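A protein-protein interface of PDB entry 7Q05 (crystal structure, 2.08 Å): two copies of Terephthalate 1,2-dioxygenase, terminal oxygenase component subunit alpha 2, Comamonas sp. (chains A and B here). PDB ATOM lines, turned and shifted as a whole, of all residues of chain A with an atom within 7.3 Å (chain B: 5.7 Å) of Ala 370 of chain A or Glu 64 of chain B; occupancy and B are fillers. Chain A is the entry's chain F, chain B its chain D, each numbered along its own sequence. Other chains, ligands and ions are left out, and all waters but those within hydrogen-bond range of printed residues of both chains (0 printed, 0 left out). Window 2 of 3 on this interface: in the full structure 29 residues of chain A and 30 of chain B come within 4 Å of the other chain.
Among the printed residues, merely in contact across the chains: Arg 367 of chain A with Pro 66 of chain B, Gly 371 of chain A with Arg 38 of chain B, Gly 371 of chain A with Glu 64 of chain B and Gly 371 of chain A with Thr 65 of chain B.
No position is printed for both chains.
Gln 366 of chain A touches none of the printed residues of chain B. Of the printed residues of chain B, Arg 367 of chain A touches Pro 66 (3.9 Å). Ala 370 of chain A touches just one residue of chain B: Glu 64. Printed residues of chain A within 4 Å of Arg 38 of chain B: Gly 371 (3.4 Å). Glu 64 of chain B touches just these residues of chain A: Ala 370 (3.3 Å) and Gly 371 (3.7 Å). Printed residues of chain A within 4 Å of Thr 65 of chain B: Gly 371. Printed residues of chain A within 4 Å of Pro 66 of chain B: Arg 367 (3.9 Å). The nearest residue of chain B that does not touch Ala 370 of chain A is Pro 66 of chain B (4.5 Å). The nearest residue of chain A that does not touch Glu 64 of chain B is Ala 372 of chain A (5.4 Å).
The backbone carbonyl oxygen (O) of Ala 370 of chain A sits close to the side-chain carboxylate (OE2) of Glu 64 of chain B (3.4 Å).
Of the 11 printed residues of chain B, 4 touch a printed residue of chain A. Of the 11 printed residues of chain A, 3 touch a printed residue of chain B. Hydrophobic or aromatic side chains of chain A within 4 Å of the printed part of chain B: Ala 370. Among the printed residues, 5 pairs touch across the chains.
OE2 of Glu 64 of chain B lies within salt-bridge range of NH2 of Arg 38 of chain B (2.9 Å). The backbone NH (N) of Arg 38 of chain B is in hydrogen-bond range of the backbone carbonyl oxygen (O) of Gln 33 of chain B (2.9 Å). N of Glu 64 of chain B is in hydrogen-bond range of OE1 of Gln 33 of chain B (2.9 Å). OG1 of Thr 65 of chain B is in hydrogen-bond range of NH2 of Arg 38 of chain B.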
ATOM      1  N   THR A  24      16.270  13.895  -5.311  1.00  0.00           N
ATOM      2  CA  THR A  24      16.760  15.223  -5.781  1.00  0.00           C
ATOM      3  C   THR A  24      17.963  15.773  -5.008  1.00  0.00           C
ATOM      4  O   THR A  24      18.607  16.685  -5.537  1.00  0.00           O
ATOM      5  CB  THR A  24      15.643  16.264  -5.774  1.00  0.00           C
ATOM      6  OG1 THR A  24      15.158  16.338  -4.440  1.00  0.00           O
ATOM      7  CG2 THR A  24      14.523  15.920  -6.729  1.00  0.00           C
ATOM      8  N   PHE A 364       7.425  10.442 -14.615  1.00  0.00           N
ATOM      9  CA  PHE A 364       6.119  10.885 -14.083  1.00  0.00           C
ATOM     10  C   PHE A 364       6.284  11.141 -12.574  1.00  0.00           C
ATOM     11  O   PHE A 364       5.703  12.100 -12.078  1.00  0.00           O
ATOM     12  CB  PHE A 364       5.012   9.896 -14.457  1.00  0.00           C
ATOM     13  CG  PHE A 364       4.776   9.733 -15.941  1.00  0.00           C
ATOM     14  CD1 PHE A 364       5.260  10.652 -16.864  1.00  0.00           C
ATOM     15  CD2 PHE A 364       4.056   8.655 -16.415  1.00  0.00           C
ATOM     16  CE1 PHE A 364       4.986  10.529 -18.218  1.00  0.00           C
ATOM     17  CE2 PHE A 364       3.831   8.497 -17.776  1.00  0.00           C
ATOM     18  CZ  PHE A 364       4.291   9.434 -18.674  1.00  0.00           C
ATOM     19  N   VAL A 365       7.071  10.317 -11.875  1.00  0.00           N
ATOM     20  CA  VAL A 365       7.334  10.451 -10.413  1.00  0.00           C
ATOM     21  C   VAL A 365       8.223  11.676 -10.220  1.00  0.00           C
ATOM     22  O   VAL A 365       7.849  12.567  -9.422  1.00  0.00           O
ATOM     23  CB  VAL A 365       7.957   9.172  -9.799  1.00  0.00           C
ATOM     24  CG1 VAL A 365       8.420   9.387  -8.366  1.00  0.00           C
ATOM     25  CG2 VAL A 365       6.979   8.006  -9.834  1.00  0.00           C
ATOM     26  N   GLN A 366       9.333  11.724 -10.952  1.00  0.00           N
ATOM     27  CA  GLN A 366      10.300  12.832 -10.878  1.00  0.00           C
ATOM     28  C   GLN A 366       9.531  14.161 -10.957  1.00  0.00           C
ATOM     29  O   GLN A 366       9.806  15.069 -10.122  1.00  0.00           O
ATOM     30  CB  GLN A 366      11.395  12.672 -11.942  1.00  0.00           C
ATOM     31  CG  GLN A 366      12.604  13.551 -11.669  1.00  0.00           C
ATOM     32  CD  GLN A 366      13.628  12.892 -10.786  1.00  0.00           C
ATOM     33  OE1 GLN A 366      13.943  11.723 -10.910  1.00  0.00           O
ATOM     34  NE2 GLN A 366      14.210  13.664  -9.890  1.00  0.00           N
ATOM     35  N   ARG A 367       8.547  14.256 -11.842  1.00  0.00           N
ATOM     36  CA  ARG A 367       7.786  15.508 -12.059  1.00  0.00           C
ATOM     37  C   ARG A 367       6.649  15.652 -11.056  1.00  0.00           C
ATOM     38  O   ARG A 367       6.363  16.828 -10.660  1.00  0.00           O
ATOM     39  CB  ARG A 367       7.283  15.559 -13.507  1.00  0.00           C
ATOM     40  CG  ARG A 367       8.383  15.931 -14.489  1.00  0.00           C
ATOM     41  CD  ARG A 367       8.161  15.444 -15.890  1.00  0.00           C
ATOM     42  NE  ARG A 367       7.007  16.033 -16.491  1.00  0.00           N
ATOM     43  CZ  ARG A 367       6.322  15.517 -17.524  1.00  0.00           C
ATOM     44  NH1 ARG A 367       5.255  16.107 -17.996  1.00  0.00           N
ATOM     45  NH2 ARG A 367       6.713  14.414 -18.112  1.00  0.00           N
ATOM     46  N   GLY A 368       5.954  14.554 -10.716  1.00  0.00           N
ATOM     47  CA  GLY A 368       4.840  14.642  -9.759  1.00  0.00           C
ATOM     48  C   GLY A 368       5.299  15.159  -8.396  1.00  0.00           C
ATOM     49  O   GLY A 368       4.504  15.810  -7.708  1.00  0.00           O
ATOM     50  N   ILE A 369       6.543  14.876  -8.023  1.00  0.00           N
ATOM     51  CA  ILE A 369       7.108  15.251  -6.693  1.00  0.00           C
ATOM     52  C   ILE A 369       7.833  16.596  -6.746  1.00  0.00           C
ATOM     53  O   ILE A 369       8.430  16.941  -5.726  1.00  0.00           O
ATOM     54  CB  ILE A 369       8.035  14.140  -6.152  1.00  0.00           C
ATOM     55  CG1 ILE A 369       9.301  13.997  -6.983  1.00  0.00           C
ATOM     56  CG2 ILE A 369       7.299  12.823  -6.027  1.00  0.00           C
ATOM     57  CD1 ILE A 369      10.273  12.982  -6.480  1.00  0.00           C
ATOM     58  N   ALA A 370       7.752  17.356  -7.838  1.00  0.00           N
ATOM     59  CA  ALA A 370       8.467  18.652  -8.001  1.00  0.00           C
ATOM     60  C   ALA A 370       8.212  19.589  -6.812  1.00  0.00           C
ATOM     61  O   ALA A 370       9.165  20.251  -6.385  1.00  0.00           O
ATOM     62  CB  ALA A 370       8.114  19.336  -9.325  1.00  0.00           C
ATOM     63  N   GLY A 371       6.990  19.638  -6.279  1.00  0.00           N
ATOM     64  CA  GLY A 371       6.644  20.518  -5.143  1.00  0.00           C
ATOM     65  C   GLY A 371       6.644  19.797  -3.793  1.00  0.00           C
ATOM     66  O   GLY A 371       6.186  20.406  -2.790  1.00  0.00           O
ATOM     67  N   ALA A 372       7.126  18.553  -3.734  1.00  0.00           N
ATOM     68  CA  ALA A 372       6.876  17.666  -2.578  1.00  0.00           C
ATOM     69  C   ALA A 372       8.189  17.035  -2.077  1.00  0.00           C
ATOM     70  O   ALA A 372       8.118  15.922  -1.556  1.00  0.00           O
ATOM     71  CB  ALA A 372       5.885  16.618  -2.985  1.00  0.00           C
ATOM     72  N   ALA A 373       9.330  17.720  -2.222  1.00  0.00           N
ATOM     73  CA  ALA A 373      10.628  17.217  -1.740  1.00  0.00           C
ATOM     74  C   ALA A 373      10.530  16.837  -0.245  1.00  0.00           C
ATOM     75  O   ALA A 373      11.304  15.935   0.157  1.00  0.00           O
ATOM     76  CB  ALA A 373      11.727  18.218  -2.021  1.00  0.00           C
ATOM     77  N   ASP B  30      13.989  28.138  -3.819  1.00  0.00           N
ATOM     78  CA  ASP B  30      13.200  27.077  -3.149  1.00  0.00           C
ATOM     79  C   ASP B  30      12.333  27.728  -2.051  1.00  0.00           C
ATOM     80  O   ASP B  30      11.163  27.317  -1.903  1.00  0.00           O
ATOM     81  CB  ASP B  30      14.074  25.933  -2.630  1.00  0.00           C
ATOM     82  CG  ASP B  30      13.198  24.818  -2.068  1.00  0.00           C
ATOM     83  OD1 ASP B  30      12.299  24.369  -2.773  1.00  0.00           O
ATOM     84  OD2 ASP B  30      13.343  24.479  -0.895  1.00  0.00           O
ATOM     85  N   GLN B  33       9.186  28.981  -3.507  1.00  0.00           N
ATOM     86  CA  GLN B  33       8.176  27.900  -3.697  1.00  0.00           C
ATOM     87  C   GLN B  33       7.418  27.664  -2.376  1.00  0.00           C
ATOM     88  O   GLN B  33       6.171  27.642  -2.384  1.00  0.00           O
ATOM     89  CB  GLN B  33       8.866  26.631  -4.196  1.00  0.00           C
ATOM     90  CG  GLN B  33       9.551  26.810  -5.534  1.00  0.00           C
ATOM     91  CD  GLN B  33       8.607  27.106  -6.676  1.00  0.00           C
ATOM     92  OE1 GLN B  33       7.400  26.841  -6.636  1.00  0.00           O
ATOM     93  NE2 GLN B  33       9.173  27.663  -7.733  1.00  0.00           N
ATOM     94  N   TYR B  37       4.596  30.645  -3.642  1.00  0.00           N
ATOM     95  CA  TYR B  37       3.669  29.888  -4.519  1.00  0.00           C
ATOM     96  C   TYR B  37       2.783  28.963  -3.667  1.00  0.00           C
ATOM     97  O   TYR B  37       1.568  28.917  -3.950  1.00  0.00           O
ATOM     98  CB  TYR B  37       4.449  29.185  -5.636  1.00  0.00           C
ATOM     99  CG  TYR B  37       5.105  30.109  -6.627  1.00  0.00           C
ATOM    100  CD1 TYR B  37       4.358  30.840  -7.522  1.00  0.00           C
ATOM    101  CD2 TYR B  37       6.481  30.270  -6.659  1.00  0.00           C
ATOM    102  CE1 TYR B  37       4.960  31.710  -8.419  1.00  0.00           C
ATOM    103  CE2 TYR B  37       7.099  31.113  -7.574  1.00  0.00           C
ATOM    104  CZ  TYR B  37       6.335  31.839  -8.462  1.00  0.00           C
ATOM    105  OH  TYR B  37       6.934  32.671  -9.377  1.00  0.00           O
ATOM    106  N   ARG B  38       3.332  28.298  -2.636  1.00  0.00           N
ATOM    107  CA  ARG B  38       2.539  27.463  -1.675  1.00  0.00           C
ATOM    108  C   ARG B  38       2.244  28.258  -0.388  1.00  0.00           C
ATOM    109  O   ARG B  38       1.821  27.663   0.581  1.00  0.00           O
ATOM    110  CB  ARG B  38       3.256  26.142  -1.372  1.00  0.00           C
ATOM    111  CG  ARG B  38       3.513  25.292  -2.612  1.00  0.00           C
ATOM    112  CD  ARG B  38       3.866  23.840  -2.336  1.00  0.00           C
ATOM    113  NE  ARG B  38       5.193  23.738  -1.762  1.00  0.00           N
ATOM    114  CZ  ARG B  38       6.349  23.739  -2.436  1.00  0.00           C
ATOM    115  NH1 ARG B  38       7.484  23.646  -1.781  1.00  0.00           N
ATOM    116  NH2 ARG B  38       6.398  23.813  -3.747  1.00  0.00           N
ATOM    117  N   PHE B  61       0.380  24.746 -13.401  1.00  0.00           N
ATOM    118  CA  PHE B  61       1.338  24.780 -12.281  1.00  0.00           C
ATOM    119  C   PHE B  61       0.907  25.895 -11.342  1.00  0.00           C
ATOM    120  O   PHE B  61       0.308  26.839 -11.784  1.00  0.00           O
ATOM    121  CB  PHE B  61       2.756  24.996 -12.799  1.00  0.00           C
ATOM    122  CG  PHE B  61       3.399  23.817 -13.483  1.00  0.00           C
ATOM    123  CD1 PHE B  61       3.273  23.638 -14.859  1.00  0.00           C
ATOM    124  CD2 PHE B  61       4.246  22.963 -12.761  1.00  0.00           C
ATOM    125  CE1 PHE B  61       3.927  22.585 -15.501  1.00  0.00           C
ATOM    126  CE2 PHE B  61       4.862  21.887 -13.403  1.00  0.00           C
ATOM    127  CZ  PHE B  61       4.701  21.700 -14.778  1.00  0.00           C
ATOM    128  N   ALA B  62       1.208  25.739 -10.067  1.00  0.00           N
ATOM    129  CA  ALA B  62       1.314  26.843  -9.092  1.00  0.00           C
ATOM    130  C   ALA B  62       2.787  26.845  -8.686  1.00  0.00           C
ATOM    131  O   ALA B  62       3.219  25.930  -7.952  1.00  0.00           O
ATOM    132  CB  ALA B  62       0.371  26.641  -7.906  1.00  0.00           C
ATOM    133  N   GLY B  63       3.540  27.819  -9.166  1.00  0.00           N
ATOM    134  CA  GLY B  63       5.018  27.750  -9.107  1.00  0.00           C
ATOM    135  C   GLY B  63       5.534  26.501  -9.806  1.00  0.00           C
ATOM    136  O   GLY B  63       5.096  26.249 -10.972  1.00  0.00           O
ATOM    137  N   GLU B  64       6.383  25.739  -9.112  1.00  0.00           N
ATOM    138  CA  GLU B  64       6.963  24.457  -9.590  1.00  0.00           C
ATOM    139  C   GLU B  64       5.946  23.309  -9.472  1.00  0.00           C
ATOM    140  O   GLU B  64       6.221  22.240 -10.015  1.00  0.00           O
ATOM    141  CB  GLU B  64       8.235  24.127  -8.786  1.00  0.00           C
ATOM    142  CG  GLU B  64       7.945  23.618  -7.371  1.00  0.00           C
ATOM    143  CD  GLU B  64       9.124  23.529  -6.395  1.00  0.00           C
ATOM    144  OE1 GLU B  64      10.260  23.565  -6.884  1.00  0.00           O
ATOM    145  OE2 GLU B  64       8.871  23.415  -5.150  1.00  0.00           O
ATOM    146  N   THR B  65       4.843  23.479  -8.742  1.00  0.00           N
ATOM    147  CA  THR B  65       3.967  22.340  -8.332  1.00  0.00           C
ATOM    148  C   THR B  65       2.907  22.106  -9.401  1.00  0.00           C
ATOM    149  O   THR B  65       2.109  22.999  -9.638  1.00  0.00           O
ATOM    150  CB  THR B  65       3.275  22.570  -6.975  1.00  0.00           C
ATOM    151  OG1 THR B  65       4.291  22.832  -6.008  1.00  0.00           O
ATOM    152  CG2 THR B  65       2.428  21.384  -6.566  1.00  0.00           C
ATOM    153  N   PRO B  66       2.837  20.911 -10.043  1.00  0.00           N
ATOM    154  CA  PRO B  66       1.821  20.640 -11.078  1.00  0.00           C
ATOM    155  C   PRO B  66       0.436  20.560 -10.419  1.00  0.00           C
ATOM    156  O   PRO B  66       0.335  20.116  -9.296  1.00  0.00           O
ATOM    157  CB  PRO B  66       2.283  19.317 -11.694  1.00  0.00           C
ATOM    158  CG  PRO B  66       2.911  18.606 -10.527  1.00  0.00           C
ATOM    159  CD  PRO B  66       3.638  19.708  -9.750  1.00  0.00           C
ATOM    160  N   PRO B 315       7.599  30.193 -12.825  1.00  0.00           N
ATOM    161  CA  PRO B 315       9.027  29.986 -12.657  1.00  0.00           C
ATOM    162  C   PRO B 315       9.358  28.613 -13.245  1.00  0.00           C
ATOM    163  O   PRO B 315       8.494  27.721 -13.149  1.00  0.00           O
ATOM    164  CB  PRO B 315       9.222  30.028 -11.140  1.00  0.00           C
ATOM    165  CG  PRO B 315       7.941  29.435 -10.646  1.00  0.00           C
ATOM    166  CD  PRO B 315       6.858  29.952 -11.585  1.00  0.00           C
